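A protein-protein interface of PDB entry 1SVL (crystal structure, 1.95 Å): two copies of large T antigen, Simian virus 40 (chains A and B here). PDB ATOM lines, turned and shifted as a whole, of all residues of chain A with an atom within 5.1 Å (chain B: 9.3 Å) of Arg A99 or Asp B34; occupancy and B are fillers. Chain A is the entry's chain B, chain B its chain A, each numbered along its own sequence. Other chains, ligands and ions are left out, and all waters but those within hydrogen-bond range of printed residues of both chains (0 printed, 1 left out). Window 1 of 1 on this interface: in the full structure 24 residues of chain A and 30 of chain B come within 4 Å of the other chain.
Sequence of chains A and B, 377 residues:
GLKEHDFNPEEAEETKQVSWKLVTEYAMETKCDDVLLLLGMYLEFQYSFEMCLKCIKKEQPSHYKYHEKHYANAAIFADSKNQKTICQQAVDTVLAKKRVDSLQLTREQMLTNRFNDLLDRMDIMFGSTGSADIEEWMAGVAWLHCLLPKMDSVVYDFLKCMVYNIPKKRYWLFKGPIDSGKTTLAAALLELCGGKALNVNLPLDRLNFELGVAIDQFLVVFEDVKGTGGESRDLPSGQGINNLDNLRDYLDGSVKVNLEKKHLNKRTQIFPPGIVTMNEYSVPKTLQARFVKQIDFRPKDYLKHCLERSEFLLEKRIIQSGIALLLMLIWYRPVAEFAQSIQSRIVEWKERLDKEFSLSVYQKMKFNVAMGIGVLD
Of the 13 printed residues of chain A, 4 touch a printed residue of chain B. Hydrophobic or aromatic side chains of chain A that line the printed part of chain B: Ala A96, Val A100 and Leu A103. Among the printed residues, Asp or Glu carboxylates within 4 Å of a Lys or Arg side-chain nitrogen of the other chain: Arg A99 with Asp B34 (3.0 Å).
Leu B36 touches Ala A96 (O to CB, 3.2 Å). Leu B39 touches Ala A96. Ala A96 touches Gly B40. Arg A99 touches Leu B36 (CG to CB, 3.6 Å). CG of Arg A99 touches N of Leu B37, at 3.8 Å. Gly B40 touches Val A100 (CA to CG2, 3.9 Å). OE2 of Glu B44 touches CG1 of Val A100, 3.8 Å away. Leu A103 touches Leu B37 (CD1 to CD2, 3.7 Å).
O of Asp B34 is in hydrogen-bond range of SG of Cys B32 (3.4 Å). The side-chain carboxylate (OD1) of Asp B34 is in hydrogen-bond range of the backbone NH (N) of Leu B36, 3.0 Å away. The side-chain carboxylate (OD1) of Asp B34 is in hydrogen-bond range of the backbone NH (N) of Leu B37, 3.2 Å away. NH2 of Arg A99 is in salt-bridge range of OD1 of Asp A216 (2.9 Å).
The side-chain carboxylate of Asp B34 lies within salt-bridge range of the guanidinium group of Arg A99 (3.0 Å).
2 positions are printed for both chains. Of the 9 pairs that touch across the chains among the printed residues, none has its exchanged pair printed and touching as well.
Leu A95 touches none of the printed residues of chain B. Of chain B, only Leu B36, Leu B39 and Gly B40 come within 4 Å of Ala A96. Of chain B, only Asp B34, Leu B36 and Leu B37 come within 4 Å of Arg A99. Printed residues of chain B within 4 Å of Leu A103: Leu B37 (3.7 Å). Asp B34 touches just one residue of chain A: Arg A99 (3.0 Å). Of the printed residues of chain A, Leu B39 touches Ala A96.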
ATOM      1  N   LEU A  95      21.818   0.960  19.473  1.00  0.00           N
ATOM      2  CA  LEU A  95      21.902   0.346  18.142  1.00  0.00           C
ATOM      3  C   LEU A  95      20.849  -0.774  17.970  1.00  0.00           C
ATOM      4  O   LEU A  95      20.262  -0.935  16.896  1.00  0.00           O
ATOM      5  CB  LEU A  95      23.309  -0.223  17.917  1.00  0.00           C
ATOM      6  CG  LEU A  95      24.444   0.800  17.875  1.00  0.00           C
ATOM      7  CD1 LEU A  95      25.773   0.071  17.785  1.00  0.00           C
ATOM      8  CD2 LEU A  95      24.254   1.756  16.691  1.00  0.00           C
ATOM      9  N   ALA A  96      20.612  -1.534  19.040  1.00  0.00           N
ATOM     10  CA  ALA A  96      19.616  -2.618  19.032  1.00  0.00           C
ATOM     11  C   ALA A  96      18.209  -2.062  18.792  1.00  0.00           C
ATOM     12  O   ALA A  96      17.427  -2.613  18.017  1.00  0.00           O
ATOM     13  CB  ALA A  96      19.663  -3.366  20.354  1.00  0.00           C
ATOM     14  N   LYS A  97      17.880  -0.959  19.461  1.00  0.00           N
ATOM     15  CA  LYS A  97      16.575  -0.341  19.284  1.00  0.00           C
ATOM     16  C   LYS A  97      16.402   0.135  17.833  1.00  0.00           C
ATOM     17  O   LYS A  97      15.312   0.031  17.275  1.00  0.00           O
ATOM     18  CB  LYS A  97      16.410   0.834  20.262  1.00  0.00           C
ATOM     19  CG  LYS A  97      15.187   1.707  20.027  1.00  0.00           C
ATOM     20  CD  LYS A  97      13.883   0.926  20.129  1.00  0.00           C
ATOM     21  CE  LYS A  97      12.664   1.851  19.987  1.00  0.00           C
ATOM     22  NZ  LYS A  97      11.373   1.112  20.128  1.00  0.00           N
ATOM     23  N   LYS A  98      17.464   0.658  17.214  1.00  0.00           N
ATOM     24  CA  LYS A  98      17.356   1.108  15.820  1.00  0.00           C
ATOM     25  C   LYS A  98      17.110  -0.132  14.947  1.00  0.00           C
ATOM     26  O   LYS A  98      16.313  -0.103  14.012  1.00  0.00           O
ATOM     27  CB  LYS A  98      18.634   1.849  15.361  1.00  0.00           C
ATOM     28  CG  LYS A  98      18.888   3.192  16.088  1.00  0.00           C
ATOM     29  CD  LYS A  98      19.904   4.115  15.389  1.00  0.00           C
ATOM     30  CE  LYS A  98      21.320   3.569  15.457  1.00  0.00           C
ATOM     31  NZ  LYS A  98      22.329   4.625  15.128  1.00  0.00           N
ATOM     32  N   ARG A  99      17.812  -1.212  15.279  1.00  0.00           N
ATOM     33  CA  ARG A  99      17.698  -2.498  14.593  1.00  0.00           C
ATOM     34  C   ARG A  99      16.227  -2.911  14.607  1.00  0.00           C
ATOM     35  O   ARG A  99      15.627  -3.174  13.574  1.00  0.00           O
ATOM     36  CB  ARG A  99      18.513  -3.549  15.349  1.00  0.00           C
ATOM     37  CG  ARG A  99      19.245  -4.567  14.500  1.00  0.00           C
ATOM     38  CD  ARG A  99      18.481  -4.965  13.266  1.00  0.00           C
ATOM     39  NE  ARG A  99      19.124  -4.391  12.088  1.00  0.00           N
ATOM     40  CZ  ARG A  99      20.379  -4.644  11.720  1.00  0.00           C
ATOM     41  NH1 ARG A  99      21.138  -5.473  12.436  1.00  0.00           N
ATOM     42  NH2 ARG A  99      20.877  -4.065  10.638  1.00  0.00           N
ATOM     43  N   VAL A 100      15.644  -2.959  15.797  1.00  0.00           N
ATOM     44  CA  VAL A 100      14.245  -3.332  15.938  1.00  0.00           C
ATOM     45  C   VAL A 100      13.298  -2.448  15.125  1.00  0.00           C
ATOM     46  O   VAL A 100      12.433  -2.945  14.394  1.00  0.00           O
ATOM     47  CB  VAL A 100      13.808  -3.272  17.410  1.00  0.00           C
ATOM     48  CG1 VAL A 100      12.303  -3.531  17.518  1.00  0.00           C
ATOM     49  CG2 VAL A 100      14.597  -4.275  18.225  1.00  0.00           C
ATOM     50  N   ASP A 101      13.436  -1.136  15.283  1.00  0.00           N
ATOM     51  CA  ASP A 101      12.575  -0.203  14.563  1.00  0.00           C
ATOM     52  C   ASP A 101      12.688  -0.412  13.058  1.00  0.00           C
ATOM     53  O   ASP A 101      11.689  -0.465  12.344  1.00  0.00           O
ATOM     54  CB  ASP A 101      12.945   1.241  14.913  1.00  0.00           C
ATOM     55  CG  ASP A 101      12.509   1.631  16.321  1.00  0.00           C
ATOM     56  OD1 ASP A 101      11.528   1.040  16.812  1.00  0.00           O
ATOM     57  OD2 ASP A 101      13.134   2.539  16.920  1.00  0.00           O
ATOM     58  N   SER A 102      13.915  -0.542  12.584  1.00  0.00           N
ATOM     59  CA  SER A 102      14.164  -0.729  11.169  1.00  0.00           C
ATOM     60  C   SER A 102      13.384  -1.936  10.607  1.00  0.00           C
ATOM     61  O   SER A 102      12.832  -1.876   9.504  1.00  0.00           O
ATOM     62  CB  SER A 102      15.668  -0.913  10.957  1.00  0.00           C
ATOM     63  OG  SER A 102      15.952  -1.120   9.588  1.00  0.00           O
ATOM     64  N   LEU A 103      13.315  -3.012  11.383  1.00  0.00           N
ATOM     65  CA  LEU A 103      12.624  -4.207  10.939  1.00  0.00           C
ATOM     66  C   LEU A 103      11.143  -4.265  11.252  1.00  0.00           C
ATOM     67  O   LEU A 103      10.399  -4.974  10.580  1.00  0.00           O
ATOM     68  CB  LEU A 103      13.291  -5.453  11.532  1.00  0.00           C
ATOM     69  CG  LEU A 103      14.741  -5.723  11.141  1.00  0.00           C
ATOM     70  CD1 LEU A 103      15.325  -6.834  12.014  1.00  0.00           C
ATOM     71  CD2 LEU A 103      14.802  -6.105   9.653  1.00  0.00           C
ATOM     72  N   ILE A 215      22.796   0.635   4.820  1.00  0.00           N
ATOM     73  CA  ILE A 215      22.158  -0.312   5.717  1.00  0.00           C
ATOM     74  C   ILE A 215      21.331   0.360   6.817  1.00  0.00           C
ATOM     75  O   ILE A 215      21.830   1.213   7.547  1.00  0.00           O
ATOM     76  CB  ILE A 215      23.212  -1.249   6.360  1.00  0.00           C
ATOM     77  CG1 ILE A 215      23.863  -2.107   5.276  1.00  0.00           C
ATOM     78  CG2 ILE A 215      22.564  -2.126   7.419  1.00  0.00           C
ATOM     79  CD1 ILE A 215      24.978  -3.009   5.777  1.00  0.00           C
ATOM     80  N   ASP A 216      20.064  -0.039   6.922  1.00  0.00           N
ATOM     81  CA  ASP A 216      19.143   0.493   7.921  1.00  0.00           C
ATOM     82  C   ASP A 216      18.710   1.941   7.664  1.00  0.00           C
ATOM     83  O   ASP A 216      17.897   2.490   8.413  1.00  0.00           O
ATOM     84  CB  ASP A 216      19.761   0.382   9.323  1.00  0.00           C
ATOM     85  CG  ASP A 216      19.825  -1.055   9.836  1.00  0.00           C
ATOM     86  OD1 ASP A 216      20.234  -1.243  11.009  1.00  0.00           O
ATOM     87  OD2 ASP A 216      19.469  -1.991   9.083  1.00  0.00           O
ATOM     88  N   ASN A 265      29.780  -4.334  10.169  1.00  0.00           N
ATOM     89  CA  ASN A 265      28.366  -4.608   9.919  1.00  0.00           C
ATOM     90  C   ASN A 265      28.101  -5.105   8.490  1.00  0.00           C
ATOM     91  O   ASN A 265      28.788  -4.712   7.541  1.00  0.00           O
ATOM     92  CB  ASN A 265      27.529  -3.355  10.197  1.00  0.00           C
ATOM     93  CG  ASN A 265      26.046  -3.645  10.239  1.00  0.00           C
ATOM     94  OD1 ASN A 265      25.465  -4.095   9.252  1.00  0.00           O
ATOM     95  ND2 ASN A 265      25.419  -3.388  11.384  1.00  0.00           N
ATOM     96  N   ARG A 267      24.523  -6.745   5.993  1.00  0.00           N
ATOM     97  CA  ARG A 267      23.086  -6.998   5.966  1.00  0.00           C
ATOM     98  C   ARG A 267      22.500  -7.033   4.558  1.00  0.00           C
ATOM     99  O   ARG A 267      22.864  -6.229   3.698  1.00  0.00           O
ATOM    100  CB  ARG A 267      22.344  -5.941   6.791  1.00  0.00           C
ATOM    101  CG  ARG A 267      20.867  -6.231   6.958  1.00  0.00           C
ATOM    102  CD  ARG A 267      20.069  -4.977   7.253  1.00  0.00           C
ATOM    103  NE  ARG A 267      18.636  -5.252   7.270  1.00  0.00           N
ATOM    104  CZ  ARG A 267      17.689  -4.318   7.259  1.00  0.00           C
ATOM    105  NH1 ARG A 267      18.015  -3.034   7.228  1.00  0.00           N
ATOM    106  NH2 ARG A 267      16.412  -4.670   7.277  1.00  0.00           N
ATOM    107  N   TYR B  26      14.033 -18.068  23.661  1.00  0.00           N
ATOM    108  CA  TYR B  26      13.292 -17.031  22.949  1.00  0.00           C
ATOM    109  C   TYR B  26      13.885 -16.900  21.535  1.00  0.00           C
ATOM    110  O   TYR B  26      13.155 -16.858  20.554  1.00  0.00           O
ATOM    111  CB  TYR B  26      13.420 -15.680  23.670  1.00  0.00           C
ATOM    112  CG  TYR B  26      12.820 -14.533  22.873  1.00  0.00           C
ATOM    113  CD1 TYR B  26      11.446 -14.444  22.682  1.00  0.00           C
ATOM    114  CD2 TYR B  26      13.638 -13.571  22.274  1.00  0.00           C
ATOM    115  CE1 TYR B  26      10.898 -13.437  21.919  1.00  0.00           C
ATOM    116  CE2 TYR B  26      13.093 -12.550  21.503  1.00  0.00           C
ATOM    117  CZ  TYR B  26      11.726 -12.491  21.329  1.00  0.00           C
ATOM    118  OH  TYR B  26      11.152 -11.486  20.567  1.00  0.00           O
ATOM    119  N   ALA B  27      15.209 -16.827  21.453  1.00  0.00           N
ATOM    120  CA  ALA B  27      15.902 -16.687  20.173  1.00  0.00           C
ATOM    121  C   ALA B  27      15.528 -17.841  19.240  1.00  0.00           C
ATOM    122  O   ALA B  27      15.259 -17.659  18.032  1.00  0.00           O
ATOM    123  CB  ALA B  27      17.402 -16.666  20.396  1.00  0.00           C
ATOM    124  N   THR B  30      11.817 -17.652  17.919  1.00  0.00           N
ATOM    125  CA  THR B  30      11.589 -16.617  16.920  1.00  0.00           C
ATOM    126  C   THR B  30      12.580 -16.692  15.756  1.00  0.00           C
ATOM    127  O   THR B  30      12.527 -15.867  14.848  1.00  0.00           O
ATOM    128  CB  THR B  30      11.680 -15.212  17.581  1.00  0.00           C
ATOM    129  OG1 THR B  30      12.944 -15.080  18.241  1.00  0.00           O
ATOM    130  CG2 THR B  30      10.559 -15.030  18.608  1.00  0.00           C
ATOM    131  N   LYS B  31      13.469 -17.684  15.793  1.00  0.00           N
ATOM    132  CA  LYS B  31      14.486 -17.884  14.749  1.00  0.00           C
ATOM    133  C   LYS B  31      15.356 -16.642  14.619  1.00  0.00           C
ATOM    134  O   LYS B  31      15.729 -16.243  13.514  1.00  0.00           O
ATOM    135  CB  LYS B  31      13.819 -18.145  13.400  1.00  0.00           C
ATOM    136  CG  LYS B  31      12.643 -19.058  13.485  1.00  0.00           C
ATOM    137  CD  LYS B  31      13.073 -20.431  13.938  1.00  0.00           C
ATOM    138  CE  LYS B  31      13.123 -21.390  12.746  1.00  0.00           C
ATOM    139  NZ  LYS B  31      11.808 -21.416  12.020  1.00  0.00           N
ATOM    140  N   CYS B  32      15.687 -16.037  15.749  1.00  0.00           N
ATOM    141  CA  CYS B  32      16.483 -14.819  15.730  1.00  0.00           C
ATOM    142  C   CYS B  32      17.977 -15.067  15.628  1.00  0.00           C
ATOM    143  O   CYS B  32      18.607 -15.538  16.577  1.00  0.00           O
ATOM    144  CB  CYS B  32      16.171 -13.992  16.972  1.00  0.00           C
ATOM    145  SG  CYS B  32      17.002 -12.412  16.976  1.00  0.00           S
ATOM    146  N   ASP B  33      18.547 -14.776  14.463  1.00  0.00           N
ATOM    147  CA  ASP B  33      19.985 -14.957  14.261  1.00  0.00           C
ATOM    148  C   ASP B  33      20.732 -13.614  14.144  1.00  0.00           C
ATOM    149  O   ASP B  33      21.847 -13.566  13.640  1.00  0.00           O
ATOM    150  CB  ASP B  33      20.269 -15.809  13.017  1.00  0.00           C
ATOM    151  CG  ASP B  33      19.712 -15.201  11.740  1.00  0.00           C
ATOM    152  OD1 ASP B  33      20.056 -15.712  10.647  1.00  0.00           O
ATOM    153  OD2 ASP B  33      18.930 -14.228  11.812  1.00  0.00           O
ATOM    154  N   ASP B  34      20.110 -12.546  14.635  1.00  0.00           N
ATOM    155  CA  ASP B  34      20.677 -11.178  14.617  1.00  0.00           C
ATOM    156  C   ASP B  34      20.892 -10.783  16.074  1.00  0.00           C
ATOM    157  O   ASP B  34      19.916 -10.597  16.777  1.00  0.00           O
ATOM    158  CB  ASP B  34      19.662 -10.212  13.994  1.00  0.00           C
ATOM    159  CG  ASP B  34      20.204  -8.779  13.839  1.00  0.00           C
ATOM    160  OD1 ASP B  34      21.058  -8.344  14.648  1.00  0.00           O
ATOM    161  OD2 ASP B  34      19.749  -8.083  12.898  1.00  0.00           O
ATOM    162  N   VAL B  35      22.139 -10.636  16.511  1.00  0.00           N
ATOM    163  CA  VAL B  35      22.420 -10.297  17.903  1.00  0.00           C
ATOM    164  C   VAL B  35      21.825  -8.964  18.374  1.00  0.00           C
ATOM    165  O   VAL B  35      21.336  -8.875  19.500  1.00  0.00           O
ATOM    166  CB  VAL B  35      23.933 -10.313  18.192  1.00  0.00           C
ATOM    167  CG1 VAL B  35      24.193  -9.984  19.670  1.00  0.00           C
ATOM    168  CG2 VAL B  35      24.496 -11.701  17.896  1.00  0.00           C
ATOM    169  N   LEU B  36      21.856  -7.938  17.520  1.00  0.00           N
ATOM    170  CA  LEU B  36      21.290  -6.639  17.903  1.00  0.00           C
ATOM    171  C   LEU B  36      19.776  -6.726  17.977  1.00  0.00           C
ATOM    172  O   LEU B  36      19.144  -6.147  18.866  1.00  0.00           O
ATOM    173  CB  LEU B  36      21.692  -5.548  16.896  1.00  0.00           C
ATOM    174  CG  LEU B  36      23.152  -5.101  16.971  1.00  0.00           C
ATOM    175  CD1 LEU B  36      23.389  -3.917  16.030  1.00  0.00           C
ATOM    176  CD2 LEU B  36      23.479  -4.704  18.414  1.00  0.00           C
ATOM    177  N   LEU B  37      19.177  -7.446  17.041  1.00  0.00           N
ATOM    178  CA  LEU B  37      17.730  -7.584  17.051  1.00  0.00           C
ATOM    179  C   LEU B  37      17.286  -8.339  18.312  1.00  0.00           C
ATOM    180  O   LEU B  37      16.264  -7.998  18.902  1.00  0.00           O
ATOM    181  CB  LEU B  37      17.240  -8.317  15.788  1.00  0.00           C
ATOM    182  CG  LEU B  37      15.785  -8.804  15.741  1.00  0.00           C
ATOM    183  CD1 LEU B  37      14.797  -7.639  15.827  1.00  0.00           C
ATOM    184  CD2 LEU B  37      15.566  -9.577  14.433  1.00  0.00           C
ATOM    185  N   LEU B  38      18.053  -9.355  18.712  1.00  0.00           N
ATOM    186  CA  LEU B  38      17.728 -10.138  19.911  1.00  0.00           C
ATOM    187  C   LEU B  38      17.831  -9.284  21.178  1.00  0.00           C
ATOM    188  O   LEU B  38      16.972  -9.346  22.053  1.00  0.00           O
ATOM    189  CB  LEU B  38      18.694 -11.310  20.059  1.00  0.00           C
ATOM    190  CG  LEU B  38      18.534 -12.121  21.355  1.00  0.00           C
ATOM    191  CD1 LEU B  38      17.086 -12.601  21.533  1.00  0.00           C
ATOM    192  CD2 LEU B  38      19.469 -13.300  21.291  1.00  0.00           C
ATOM    193  N   LEU B  39      18.913  -8.516  21.265  1.00  0.00           N
ATOM    194  CA  LEU B  39      19.161  -7.645  22.406  1.00  0.00           C
ATOM    195  C   LEU B  39      18.003  -6.660  22.559  1.00  0.00           C
ATOM    196  O   LEU B  39      17.453  -6.503  23.649  1.00  0.00           O
ATOM    197  CB  LEU B  39      20.495  -6.902  22.214  1.00  0.00           C
ATOM    198  CG  LEU B  39      20.884  -5.748  23.167  1.00  0.00           C
ATOM    199  CD1 LEU B  39      20.877  -6.252  24.602  1.00  0.00           C
ATOM    200  CD2 LEU B  39      22.265  -5.198  22.815  1.00  0.00           C
ATOM    201  N   GLY B  40      17.618  -6.012  21.460  1.00  0.00           N
ATOM    202  CA  GLY B  40      16.526  -5.052  21.504  1.00  0.00           C
ATOM    203  C   GLY B  40      15.171  -5.662  21.807  1.00  0.00           C
ATOM    204  O   GLY B  40      14.319  -5.068  22.505  1.00  0.00           O
ATOM    205  N   MET B  41      14.940  -6.853  21.270  1.00  0.00           N
ATOM    206  CA  MET B  41      13.673  -7.509  21.515  1.00  0.00           C
ATOM    207  C   MET B  41      13.567  -7.886  22.976  1.00  0.00           C
ATOM    208  O   MET B  41      12.552  -7.619  23.611  1.00  0.00           O
ATOM    209  CB  MET B  41      13.520  -8.777  20.655  1.00  0.00           C
ATOM    210  CG  MET B  41      13.141  -8.491  19.213  1.00  0.00           C
ATOM    211  SD  MET B  41      11.752  -7.336  19.136  1.00  0.00           S
ATOM    212  CE  MET B  41      10.305  -8.439  19.191  1.00  0.00           C
ATOM    213  N   TYR B  42      14.609  -8.503  23.505  1.00  0.00           N
ATOM    214  CA  TYR B  42      14.574  -8.933  24.890  1.00  0.00           C
ATOM    215  C   TYR B  42      14.439  -7.787  25.887  1.00  0.00           C
ATOM    216  O   TYR B  42      13.704  -7.899  26.865  1.00  0.00           O
ATOM    217  CB  TYR B  42      15.796  -9.759  25.229  1.00  0.00           C
ATOM    218  CG  TYR B  42      15.441 -10.901  26.162  1.00  0.00           C
ATOM    219  CD1 TYR B  42      14.701 -11.998  25.696  1.00  0.00           C
ATOM    220  CD2 TYR B  42      15.832 -10.883  27.503  1.00  0.00           C
ATOM    221  CE1 TYR B  42      14.359 -13.050  26.541  1.00  0.00           C
ATOM    222  CE2 TYR B  42      15.496 -11.931  28.367  1.00  0.00           C
ATOM    223  CZ  TYR B  42      14.759 -13.007  27.885  1.00  0.00           C
ATOM    224  OH  TYR B  42      14.397 -14.015  28.752  1.00  0.00           O
ATOM    225  N   GLU B  44      12.773  -5.234  25.676  1.00  0.00           N
ATOM    226  CA  GLU B  44      11.394  -4.752  25.716  1.00  0.00           C
ATOM    227  C   GLU B  44      10.557  -5.554  26.691  1.00  0.00           C
ATOM    228  O   GLU B  44       9.433  -5.170  27.002  1.00  0.00           O
ATOM    229  CB  GLU B  44      10.701  -4.855  24.350  1.00  0.00           C
ATOM    230  CG  GLU B  44      11.432  -4.184  23.205  1.00  0.00           C
ATOM    231  CD  GLU B  44      10.610  -4.170  21.918  1.00  0.00           C
ATOM    232  OE1 GLU B  44       9.727  -5.037  21.744  1.00  0.00           O
ATOM    233  OE2 GLU B  44      10.854  -3.291  21.068  1.00  0.00           O
ATOM    234  N   LYS B  84      25.418  -8.485  25.775  1.00  0.00           N
ATOM    235  CA  LYS B  84      25.852  -8.877  24.427  1.00  0.00           C
ATOM    236  C   LYS B  84      26.374 -10.325  24.368  1.00  0.00           C
ATOM    237  O   LYS B  84      26.116 -11.050  23.412  1.00  0.00           O
ATOM    238  CB  LYS B  84      26.944  -7.908  23.926  1.00  0.00           C
ATOM    239  CG  LYS B  84      27.298  -8.013  22.434  1.00  0.00           C
ATOM    240  CD  LYS B  84      26.597  -6.935  21.607  1.00  0.00           C
ATOM    241  CE  LYS B  84      26.979  -7.002  20.123  1.00  0.00           C
ATOM    242  NZ  LYS B  84      28.453  -6.839  19.939  1.00  0.00           N
ATOM    243  N   CYS B  87      23.388 -12.746  24.485  1.00  0.00           N
ATOM    244  CA  CYS B  87      22.695 -12.767  23.216  1.00  0.00           C
ATOM    245  C   CYS B  87      23.493 -13.499  22.145  1.00  0.00           C
ATOM    246  O   CYS B  87      22.908 -14.147  21.293  1.00  0.00           O
ATOM    247  CB  CYS B  87      22.414 -11.341  22.748  1.00  0.00           C
ATOM    248  SG  CYS B  87      21.139 -10.525  23.736  1.00  0.00           S
ATOM    249  N   GLN B  88      24.815 -13.368  22.190  1.00  0.00           N
ATOM    250  CA  GLN B  88      25.700 -14.008  21.222  1.00  0.00           C
ATOM    251  C   GLN B  88      25.603 -15.532  21.328  1.00  0.00           C
ATOM    252  O   GLN B  88      25.597 -16.235  20.315  1.00  0.00           O
ATOM    253  CB  GLN B  88      27.145 -13.578  21.449  1.00  0.00           C
ATOM    254  CG  GLN B  88      28.102 -14.059  20.374  1.00  0.00           C
ATOM    255  CD  GLN B  88      27.671 -13.587  18.999  1.00  0.00           C
ATOM    256  OE1 GLN B  88      27.332 -14.385  18.109  1.00  0.00           O
ATOM    257  NE2 GLN B  88      27.656 -12.273  18.822  1.00  0.00           N
ATOM    258  N   ALA B  90      23.028 -17.143  22.450  1.00  0.00           N
ATOM    259  CA  ALA B  90      21.687 -17.477  22.003  1.00  0.00           C
ATOM    260  C   ALA B  90      21.616 -17.477  20.474  1.00  0.00           C
ATOM    261  O   ALA B  90      20.957 -18.336  19.850  1.00  0.00           O
ATOM    262  CB  ALA B  90      20.684 -16.489  22.559  1.00  0.00           C
ATOM    263  N   VAL B  91      22.288 -16.515  19.863  1.00  0.00           N
ATOM    264  CA  VAL B  91      22.281 -16.437  18.413  1.00  0.00           C
ATOM    265  C   VAL B  91      23.128 -17.572  17.828  1.00  0.00           C
ATOM    266  O   VAL B  91      22.776 -18.135  16.802  1.00  0.00           O
ATOM    267  CB  VAL B  91      22.802 -15.053  17.932  1.00  0.00           C
ATOM    268  CG1 VAL B  91      23.319 -15.142  16.476  1.00  0.00           C
ATOM    269  CG2 VAL B  91      21.667 -14.032  18.031  1.00  0.00           C
ATOM    270  N   ASP B  92      24.236 -17.899  18.473  1.00  0.00           N
ATOM    271  CA  ASP B  92      25.092 -18.980  18.001  1.00  0.00           C
ATOM    272  C   ASP B  92      24.309 -20.307  17.979  1.00  0.00           C
ATOM    273  O   ASP B  92      24.522 -21.154  17.100  1.00  0.00           O
ATOM    274  CB  ASP B  92      26.339 -19.100  18.883  1.00  0.00           C
ATOM    275  CG  ASP B  92      27.382 -18.030  18.562  1.00  0.00           C
ATOM    276  OD1 ASP B  92      27.231 -17.338  17.522  1.00  0.00           O
ATOM    277  OD2 ASP B  92      28.353 -17.882  19.337  1.00  0.00           O
ATOM    278  N   VAL B  94      21.045 -20.569  17.458  1.00  0.00           N
ATOM    279  CA  VAL B  94      20.146 -20.528  16.319  1.00  0.00           C
ATOM    280  C   VAL B  94      20.915 -20.843  15.035  1.00  0.00           C
ATOM    281  O   VAL B  94      20.393 -21.542  14.167  1.00  0.00           O
ATOM    282  CB  VAL B  94      19.431 -19.159  16.206  1.00  0.00           C
ATOM    283  CG1 VAL B  94      18.584 -19.112  14.921  1.00  0.00           C
ATOM    284  CG2 VAL B  94      18.532 -18.931  17.428  1.00  0.00           C
ATOM    285  N   LEU B  95      22.143 -20.344  14.924  1.00  0.00           N
ATOM    286  CA  LEU B  95      22.982 -20.595  13.756  1.00  0.00           C
ATOM    287  C   LEU B  95      23.415 -22.069  13.725  1.00  0.00           C
ATOM    288  O   LEU B  95      23.482 -22.681  12.663  1.00  0.00           O
ATOM    289  CB  LEU B  95      24.231 -19.717  13.778  1.00  0.00           C
ATOM    290  CG  LEU B  95      24.020 -18.212  13.577  1.00  0.00           C
ATOM    291  CD1 LEU B  95      25.355 -17.500  13.765  1.00  0.00           C
ATOM    292  CD2 LEU B  95      23.442 -17.949  12.185  1.00  0.00           C
ATOM    293  N   LYS B  98      20.602 -24.112  12.408  1.00  0.00           N
ATOM    294  CA  LYS B  98      20.473 -23.929  10.970  1.00  0.00           C
ATOM    295  C   LYS B  98      21.517 -24.786  10.245  1.00  0.00           C
ATOM    296  O   LYS B  98      21.218 -25.406   9.225  1.00  0.00           O
ATOM    297  CB  LYS B  98      20.613 -22.435  10.629  1.00  0.00           C
ATOM    298  CG  LYS B  98      19.359 -21.623  10.982  1.00  0.00           C
ATOM    299  CD  LYS B  98      19.598 -20.096  10.913  1.00  0.00           C
ATOM    300  CE  LYS B  98      18.319 -19.308  10.566  1.00  0.00           C
ATOM    301  NZ  LYS B  98      17.086 -19.802  11.267  1.00  0.00           N
